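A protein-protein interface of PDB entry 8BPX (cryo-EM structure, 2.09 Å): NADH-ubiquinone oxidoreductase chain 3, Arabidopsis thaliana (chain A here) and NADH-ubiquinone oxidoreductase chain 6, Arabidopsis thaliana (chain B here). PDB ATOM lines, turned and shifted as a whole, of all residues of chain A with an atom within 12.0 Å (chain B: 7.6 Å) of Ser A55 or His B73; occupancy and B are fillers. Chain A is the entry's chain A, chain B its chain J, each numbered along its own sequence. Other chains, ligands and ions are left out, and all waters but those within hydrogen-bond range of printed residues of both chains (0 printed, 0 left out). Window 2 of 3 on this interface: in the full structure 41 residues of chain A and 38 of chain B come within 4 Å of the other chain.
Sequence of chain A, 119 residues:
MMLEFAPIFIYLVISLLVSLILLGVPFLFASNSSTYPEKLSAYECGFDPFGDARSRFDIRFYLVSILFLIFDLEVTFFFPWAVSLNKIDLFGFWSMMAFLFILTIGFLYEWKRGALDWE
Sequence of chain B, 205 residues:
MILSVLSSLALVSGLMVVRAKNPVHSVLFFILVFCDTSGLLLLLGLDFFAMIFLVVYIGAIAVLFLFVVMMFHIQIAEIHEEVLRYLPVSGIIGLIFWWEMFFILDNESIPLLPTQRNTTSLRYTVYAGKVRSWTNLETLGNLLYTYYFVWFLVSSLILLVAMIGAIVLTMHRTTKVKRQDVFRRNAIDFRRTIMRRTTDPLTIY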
ATOM      1  N   SER A  55     -11.264 -33.365  -5.973  1.00  0.00           N
ATOM      2  CA  SER A  55     -12.151 -32.211  -5.938  1.00  0.00           C
ATOM      3  C   SER A  55     -12.216 -31.618  -4.535  1.00  0.00           C
ATOM      4  O   SER A  55     -13.240 -31.069  -4.128  1.00  0.00           O
ATOM      5  CB  SER A  55     -13.552 -32.603  -6.413  1.00  0.00           C
ATOM      6  OG  SER A  55     -14.190 -33.452  -5.475  1.00  0.00           O
ATOM      7  N   ARG A  56     -11.109 -31.730  -3.800  1.00  0.00           N
ATOM      8  CA  ARG A  56     -11.019 -31.303  -2.401  1.00  0.00           C
ATOM      9  C   ARG A  56      -9.731 -30.494  -2.244  1.00  0.00           C
ATOM     10  O   ARG A  56      -8.677 -31.049  -1.924  1.00  0.00           O
ATOM     11  CB  ARG A  56     -11.046 -32.509  -1.476  1.00  0.00           C
ATOM     12  CG  ARG A  56     -12.299 -33.362  -1.600  1.00  0.00           C
ATOM     13  CD  ARG A  56     -12.243 -34.572  -0.686  1.00  0.00           C
ATOM     14  NE  ARG A  56     -11.170 -35.484  -1.063  1.00  0.00           N
ATOM     15  CZ  ARG A  56     -11.269 -36.407  -2.011  1.00  0.00           C
ATOM     16  NH1 ARG A  56     -12.379 -36.558  -2.715  1.00  0.00           N
ATOM     17  NH2 ARG A  56     -10.228 -37.196  -2.260  1.00  0.00           N
ATOM     18  N   PHE A  57      -9.816 -29.185  -2.455  1.00  0.00           N
ATOM     19  CA  PHE A  57      -8.620 -28.352  -2.473  1.00  0.00           C
ATOM     20  C   PHE A  57      -8.147 -28.072  -1.052  1.00  0.00           C
ATOM     21  O   PHE A  57      -8.883 -27.495  -0.246  1.00  0.00           O
ATOM     22  CB  PHE A  57      -8.893 -27.045  -3.215  1.00  0.00           C
ATOM     23  CG  PHE A  57      -7.649 -26.271  -3.553  1.00  0.00           C
ATOM     24  CD1 PHE A  57      -6.996 -25.519  -2.589  1.00  0.00           C
ATOM     25  CD2 PHE A  57      -7.127 -26.307  -4.831  1.00  0.00           C
ATOM     26  CE1 PHE A  57      -5.849 -24.815  -2.897  1.00  0.00           C
ATOM     27  CE2 PHE A  57      -5.979 -25.606  -5.145  1.00  0.00           C
ATOM     28  CZ  PHE A  57      -5.339 -24.861  -4.178  1.00  0.00           C
ATOM     29  N   ASP A  58      -6.911 -28.463  -0.752  1.00  0.00           N
ATOM     30  CA  ASP A  58      -6.308 -28.243   0.558  1.00  0.00           C
ATOM     31  C   ASP A  58      -5.201 -27.206   0.386  1.00  0.00           C
ATOM     32  O   ASP A  58      -4.172 -27.484  -0.238  1.00  0.00           O
ATOM     33  CB  ASP A  58      -5.780 -29.554   1.139  1.00  0.00           C
ATOM     34  CG  ASP A  58      -5.116 -29.379   2.497  1.00  0.00           C
ATOM     35  OD1 ASP A  58      -5.063 -28.248   3.019  1.00  0.00           O
ATOM     36  OD2 ASP A  58      -4.644 -30.392   3.050  1.00  0.00           O
ATOM     37  N   ILE A  59      -5.417 -26.017   0.954  1.00  0.00           N
ATOM     38  CA  ILE A  59      -4.496 -24.896   0.807  1.00  0.00           C
ATOM     39  C   ILE A  59      -3.122 -25.173   1.398  1.00  0.00           C
ATOM     40  O   ILE A  59      -2.141 -24.547   0.987  1.00  0.00           O
ATOM     41  CB  ILE A  59      -5.107 -23.631   1.447  1.00  0.00           C
ATOM     42  CG1 ILE A  59      -5.104 -23.768   2.974  1.00  0.00           C
ATOM     43  CG2 ILE A  59      -6.493 -23.350   0.882  1.00  0.00           C
ATOM     44  CD1 ILE A  59      -5.528 -22.541   3.715  1.00  0.00           C
ATOM     45  N   PHE A  61      -1.067 -27.532   1.051  1.00  0.00           N
ATOM     46  CA  PHE A  61      -0.091 -27.973   0.061  1.00  0.00           C
ATOM     47  C   PHE A  61       0.469 -26.793  -0.723  1.00  0.00           C
ATOM     48  O   PHE A  61       1.674 -26.734  -0.995  1.00  0.00           O
ATOM     49  CB  PHE A  61      -0.726 -29.002  -0.870  1.00  0.00           C
ATOM     50  CG  PHE A  61      -1.004 -30.317  -0.205  1.00  0.00           C
ATOM     51  CD1 PHE A  61       0.036 -31.130   0.215  1.00  0.00           C
ATOM     52  CD2 PHE A  61      -2.305 -30.731   0.024  1.00  0.00           C
ATOM     53  CE1 PHE A  61      -0.217 -32.340   0.838  1.00  0.00           C
ATOM     54  CE2 PHE A  61      -2.563 -31.938   0.646  1.00  0.00           C
ATOM     55  CZ  PHE A  61      -1.518 -32.742   1.054  1.00  0.00           C
ATOM     56  N   PRO B  23      -4.482 -28.726 -18.553  1.00  0.00           N
ATOM     57  CA  PRO B  23      -3.443 -27.900 -17.847  1.00  0.00           C
ATOM     58  C   PRO B  23      -2.351 -28.669 -17.088  1.00  0.00           C
ATOM     59  O   PRO B  23      -1.264 -28.181 -17.088  1.00  0.00           O
ATOM     60  CB  PRO B  23      -4.196 -26.922 -16.927  1.00  0.00           C
ATOM     61  CG  PRO B  23      -5.625 -27.427 -16.917  1.00  0.00           C
ATOM     62  CD  PRO B  23      -5.820 -28.372 -18.090  1.00  0.00           C
ATOM     63  N   VAL B  24      -2.648 -29.841 -16.579  1.00  0.00           N
ATOM     64  CA  VAL B  24      -1.592 -30.693 -15.950  1.00  0.00           C
ATOM     65  C   VAL B  24      -0.562 -31.010 -17.043  1.00  0.00           C
ATOM     66  O   VAL B  24       0.609 -30.856 -16.780  1.00  0.00           O
ATOM     67  CB  VAL B  24      -2.117 -31.991 -15.274  1.00  0.00           C
ATOM     68  CG1 VAL B  24      -1.034 -32.986 -14.909  1.00  0.00           C
ATOM     69  CG2 VAL B  24      -3.049 -31.717 -14.105  1.00  0.00           C
ATOM     70  N   PHE B  67       1.078 -28.746  -8.091  1.00  0.00           N
ATOM     71  CA  PHE B  67       0.222 -28.916  -6.922  1.00  0.00           C
ATOM     72  C   PHE B  67      -1.072 -28.130  -7.080  1.00  0.00           C
ATOM     73  O   PHE B  67      -2.164 -28.654  -6.832  1.00  0.00           O
ATOM     74  CB  PHE B  67       0.952 -28.479  -5.649  1.00  0.00           C
ATOM     75  CG  PHE B  67       1.931 -29.489  -5.124  1.00  0.00           C
ATOM     76  CD1 PHE B  67       2.326 -30.568  -5.895  1.00  0.00           C
ATOM     77  CD2 PHE B  67       2.455 -29.357  -3.853  1.00  0.00           C
ATOM     78  CE1 PHE B  67       3.222 -31.495  -5.401  1.00  0.00           C
ATOM     79  CE2 PHE B  67       3.356 -30.278  -3.357  1.00  0.00           C
ATOM     80  CZ  PHE B  67       3.740 -31.344  -4.130  1.00  0.00           C
ATOM     81  N   VAL B  68      -0.970 -26.871  -7.505  1.00  0.00           N
ATOM     82  CA  VAL B  68      -2.169 -26.045  -7.613  1.00  0.00           C
ATOM     83  C   VAL B  68      -3.090 -26.566  -8.714  1.00  0.00           C
ATOM     84  O   VAL B  68      -4.294 -26.746  -8.502  1.00  0.00           O
ATOM     85  CB  VAL B  68      -1.791 -24.571  -7.838  1.00  0.00           C
ATOM     86  CG1 VAL B  68      -3.006 -23.777  -8.284  1.00  0.00           C
ATOM     87  CG2 VAL B  68      -1.210 -23.986  -6.563  1.00  0.00           C
ATOM     88  N   VAL B  69      -2.533 -26.866  -9.895  1.00  0.00           N
ATOM     89  CA  VAL B  69      -3.353 -27.267 -11.069  1.00  0.00           C
ATOM     90  C   VAL B  69      -3.982 -28.647 -10.830  1.00  0.00           C
ATOM     91  O   VAL B  69      -5.152 -28.769 -11.035  1.00  0.00           O
ATOM     92  CB  VAL B  69      -2.566 -27.157 -12.397  1.00  0.00           C
ATOM     93  CG1 VAL B  69      -3.254 -27.784 -13.592  1.00  0.00           C
ATOM     94  CG2 VAL B  69      -2.134 -25.732 -12.699  1.00  0.00           C
ATOM     95  N   MET B  70      -3.283 -29.510 -10.159  1.00  0.00           N
ATOM     96  CA  MET B  70      -3.810 -30.849  -9.923  1.00  0.00           C
ATOM     97  C   MET B  70      -4.991 -30.817  -8.960  1.00  0.00           C
ATOM     98  O   MET B  70      -5.987 -31.518  -9.168  1.00  0.00           O
ATOM     99  CB  MET B  70      -2.697 -31.744  -9.383  1.00  0.00           C
ATOM    100  CG  MET B  70      -1.901 -32.444 -10.467  1.00  0.00           C
ATOM    101  SD  MET B  70      -0.655 -33.558  -9.807  1.00  0.00           S
ATOM    102  CE  MET B  70       0.062 -34.182 -11.326  1.00  0.00           C
ATOM    103  N   MET B  71      -4.900 -30.011  -7.900  1.00  0.00           N
ATOM    104  CA  MET B  71      -5.992 -29.928  -6.939  1.00  0.00           C
ATOM    105  C   MET B  71      -7.172 -29.117  -7.466  1.00  0.00           C
ATOM    106  O   MET B  71      -8.268 -29.218  -6.910  1.00  0.00           O
ATOM    107  CB  MET B  71      -5.495 -29.328  -5.621  1.00  0.00           C
ATOM    108  CG  MET B  71      -4.496 -30.194  -4.873  1.00  0.00           C
ATOM    109  SD  MET B  71      -4.106 -29.559  -3.231  1.00  0.00           S
ATOM    110  CE  MET B  71      -3.374 -27.981  -3.642  1.00  0.00           C
ATOM    111  N   PHE B  72      -6.973 -28.317  -8.519  1.00  0.00           N
ATOM    112  CA  PHE B  72      -8.079 -27.569  -9.109  1.00  0.00           C
ATOM    113  C   PHE B  72      -9.080 -28.491  -9.797  1.00  0.00           C
ATOM    114  O   PHE B  72     -10.281 -28.203  -9.793  1.00  0.00           O
ATOM    115  CB  PHE B  72      -7.554 -26.537 -10.112  1.00  0.00           C
ATOM    116  CG  PHE B  72      -7.207 -25.199  -9.506  1.00  0.00           C
ATOM    117  CD1 PHE B  72      -7.556 -24.892  -8.205  1.00  0.00           C
ATOM    118  CD2 PHE B  72      -6.522 -24.250 -10.252  1.00  0.00           C
ATOM    119  CE1 PHE B  72      -7.231 -23.664  -7.653  1.00  0.00           C
ATOM    120  CE2 PHE B  72      -6.194 -23.020  -9.711  1.00  0.00           C
ATOM    121  CZ  PHE B  72      -6.548 -22.728  -8.405  1.00  0.00           C
ATOM    122  N   HIS B  73      -8.608 -29.593 -10.388  1.00  0.00           N
ATOM    123  CA  HIS B  73      -9.456 -30.526 -11.135  1.00  0.00           C
ATOM    124  C   HIS B  73     -10.296 -29.796 -12.182  1.00  0.00           C
ATOM    125  O   HIS B  73     -11.523 -29.892 -12.212  1.00  0.00           O
ATOM    126  CB  HIS B  73     -10.343 -31.340 -10.191  1.00  0.00           C
ATOM    127  CG  HIS B  73      -9.579 -32.246  -9.276  1.00  0.00           C
ATOM    128  ND1 HIS B  73      -9.337 -31.937  -7.954  1.00  0.00           N
ATOM    129  CD2 HIS B  73      -9.000 -33.450  -9.492  1.00  0.00           C
ATOM    130  CE1 HIS B  73      -8.638 -32.910  -7.398  1.00  0.00           C
ATOM    131  NE2 HIS B  73      -8.425 -33.843  -8.308  1.00  0.00           N
ATOM    132  N   ILE B  74      -9.606 -29.047 -13.011  1.00  0.00           N
ATOM    133  CA  ILE B  74     -10.306 -28.251 -14.056  1.00  0.00           C
ATOM    134  C   ILE B  74     -11.003 -29.146 -15.078  1.00  0.00           C
ATOM    135  O   ILE B  74     -10.405 -30.078 -15.544  1.00  0.00           O
ATOM    136  CB  ILE B  74      -9.381 -27.216 -14.733  1.00  0.00           C
ATOM    137  CG1 ILE B  74      -8.906 -26.190 -13.703  1.00  0.00           C
ATOM    138  CG2 ILE B  74     -10.036 -26.558 -15.923  1.00  0.00           C
ATOM    139  CD1 ILE B  74      -7.439 -25.885 -13.774  1.00  0.00           C
ATOM    140  N   GLN B  75     -12.255 -28.849 -15.332  1.00  0.00           N
ATOM    141  CA  GLN B  75     -12.975 -29.502 -16.414  1.00  0.00           C
ATOM    142  C   GLN B  75     -12.721 -28.759 -17.718  1.00  0.00           C
ATOM    143  O   GLN B  75     -12.658 -27.527 -17.742  1.00  0.00           O
ATOM    144  CB  GLN B  75     -14.473 -29.553 -16.116  1.00  0.00           C
ATOM    145  CG  GLN B  75     -14.807 -30.214 -14.789  1.00  0.00           C
ATOM    146  CD  GLN B  75     -14.020 -31.490 -14.566  1.00  0.00           C
ATOM    147  OE1 GLN B  75     -14.289 -32.517 -15.188  1.00  0.00           O
ATOM    148  NE2 GLN B  75     -13.038 -31.429 -13.673  1.00  0.00           N
ATOM    149  N   ILE B  76     -12.576 -29.520 -18.805  1.00  0.00           N
ATOM    150  CA  ILE B  76     -12.194 -28.924 -20.080  1.00  0.00           C
ATOM    151  C   ILE B  76     -13.259 -27.964 -20.592  1.00  0.00           C
ATOM    152  O   ILE B  76     -12.942 -27.004 -21.303  1.00  0.00           O
ATOM    153  CB  ILE B  76     -11.873 -30.017 -21.116  1.00  0.00           C
ATOM    154  CG1 ILE B  76     -11.258 -29.376 -22.355  1.00  0.00           C
ATOM    155  CG2 ILE B  76     -13.127 -30.790 -21.492  1.00  0.00           C
ATOM    156  CD1 ILE B  76      -9.818 -29.037 -22.176  1.00  0.00           C
ATOM    157  N   GLU B  78     -14.722 -25.687 -19.062  1.00  0.00           N
ATOM    158  CA  GLU B  78     -14.522 -24.355 -18.511  1.00  0.00           C
ATOM    159  C   GLU B  78     -13.415 -23.584 -19.220  1.00  0.00           C
ATOM    160  O   GLU B  78     -13.395 -22.351 -19.145  1.00  0.00           O
ATOM    161  CB  GLU B  78     -14.221 -24.459 -17.017  1.00  0.00           C
ATOM    162  CG  GLU B  78     -15.472 -24.576 -16.158  1.00  0.00           C
ATOM    163  CD  GLU B  78     -15.178 -25.062 -14.755  1.00  0.00           C
ATOM    164  OE1 GLU B  78     -14.074 -25.600 -14.528  1.00  0.00           O
ATOM    165  OE2 GLU B  78     -16.052 -24.908 -13.875  1.00  0.00           O
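Hydrophobic or aromatic side chains of chain A within 4 Å of the printed part of chain B: Phe A57 and Phe A61. Hydrophobic or aromatic side chains of chain B that line the printed part of chain A: Phe B67, Met B71, Phe B72 and His B73. Among the printed residues, 7 pairs touch across the chains. Among the printed residues, no Asp or Glu carboxylate lies within 4 Å of a Lys or Arg side-chain nitrogen of the other chain.
The backbone NH (N) of Ser A55 lies close to a ring nitrogen (ND1) of His B73, 3.1 Å away. The side-chain sulfur (SD) of Met B71 lies close to the backbone carbonyl oxygen (O) of Asp A58.
Phe A57 touches Val B68. CB of Met B71 touches CD2 of Phe A57, 3.5 Å away. Phe B72 touches Phe A57 (CE1 to CE2, 3.4 Å). CD2 of Phe B67 touches O of Phe A61, 3.96 Å away. Phe A61 touches Met B71 (CD2 to SD, 3.9 Å).
The backbone carbonyl oxygen (O) of His B73 sits at hydrogen-bond distance from the side-chain amide nitrogen (NE2) of Gln B75, 2.6 Å away. ND1 of His B73 sits at hydrogen-bond distance from O of Met B71. The backbone carbonyl oxygen (O) of Met B70 is in hydrogen-bond range of a ring nitrogen (NE2) of His B73 (3.5 Å).
Of chain B, only His B73 comes within 4 Å of Ser A55. Ile A59 touches none of the printed residues of chain B. Of the printed residues of chain B, Phe A61 touches Phe B67 (3.96 Å) and Met B71 (3.9 Å). Val B24 touches none of the printed residues of chain A. Of the printed residues of chain A, Phe B67 touches Phe A61. Of the printed residues of chain A, Val B68 touches Phe A57. No residue of chain A comes within 4 Å of Val B69. Of the printed residues of chain A, Met B71 touches Phe A57, Asp A58 and Phe A61. Of chain A, only Phe A57 comes within 4 Å of Phe B72. Printed residues of chain A within 4 Å of His B73: Ser A55 (3.0 Å).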
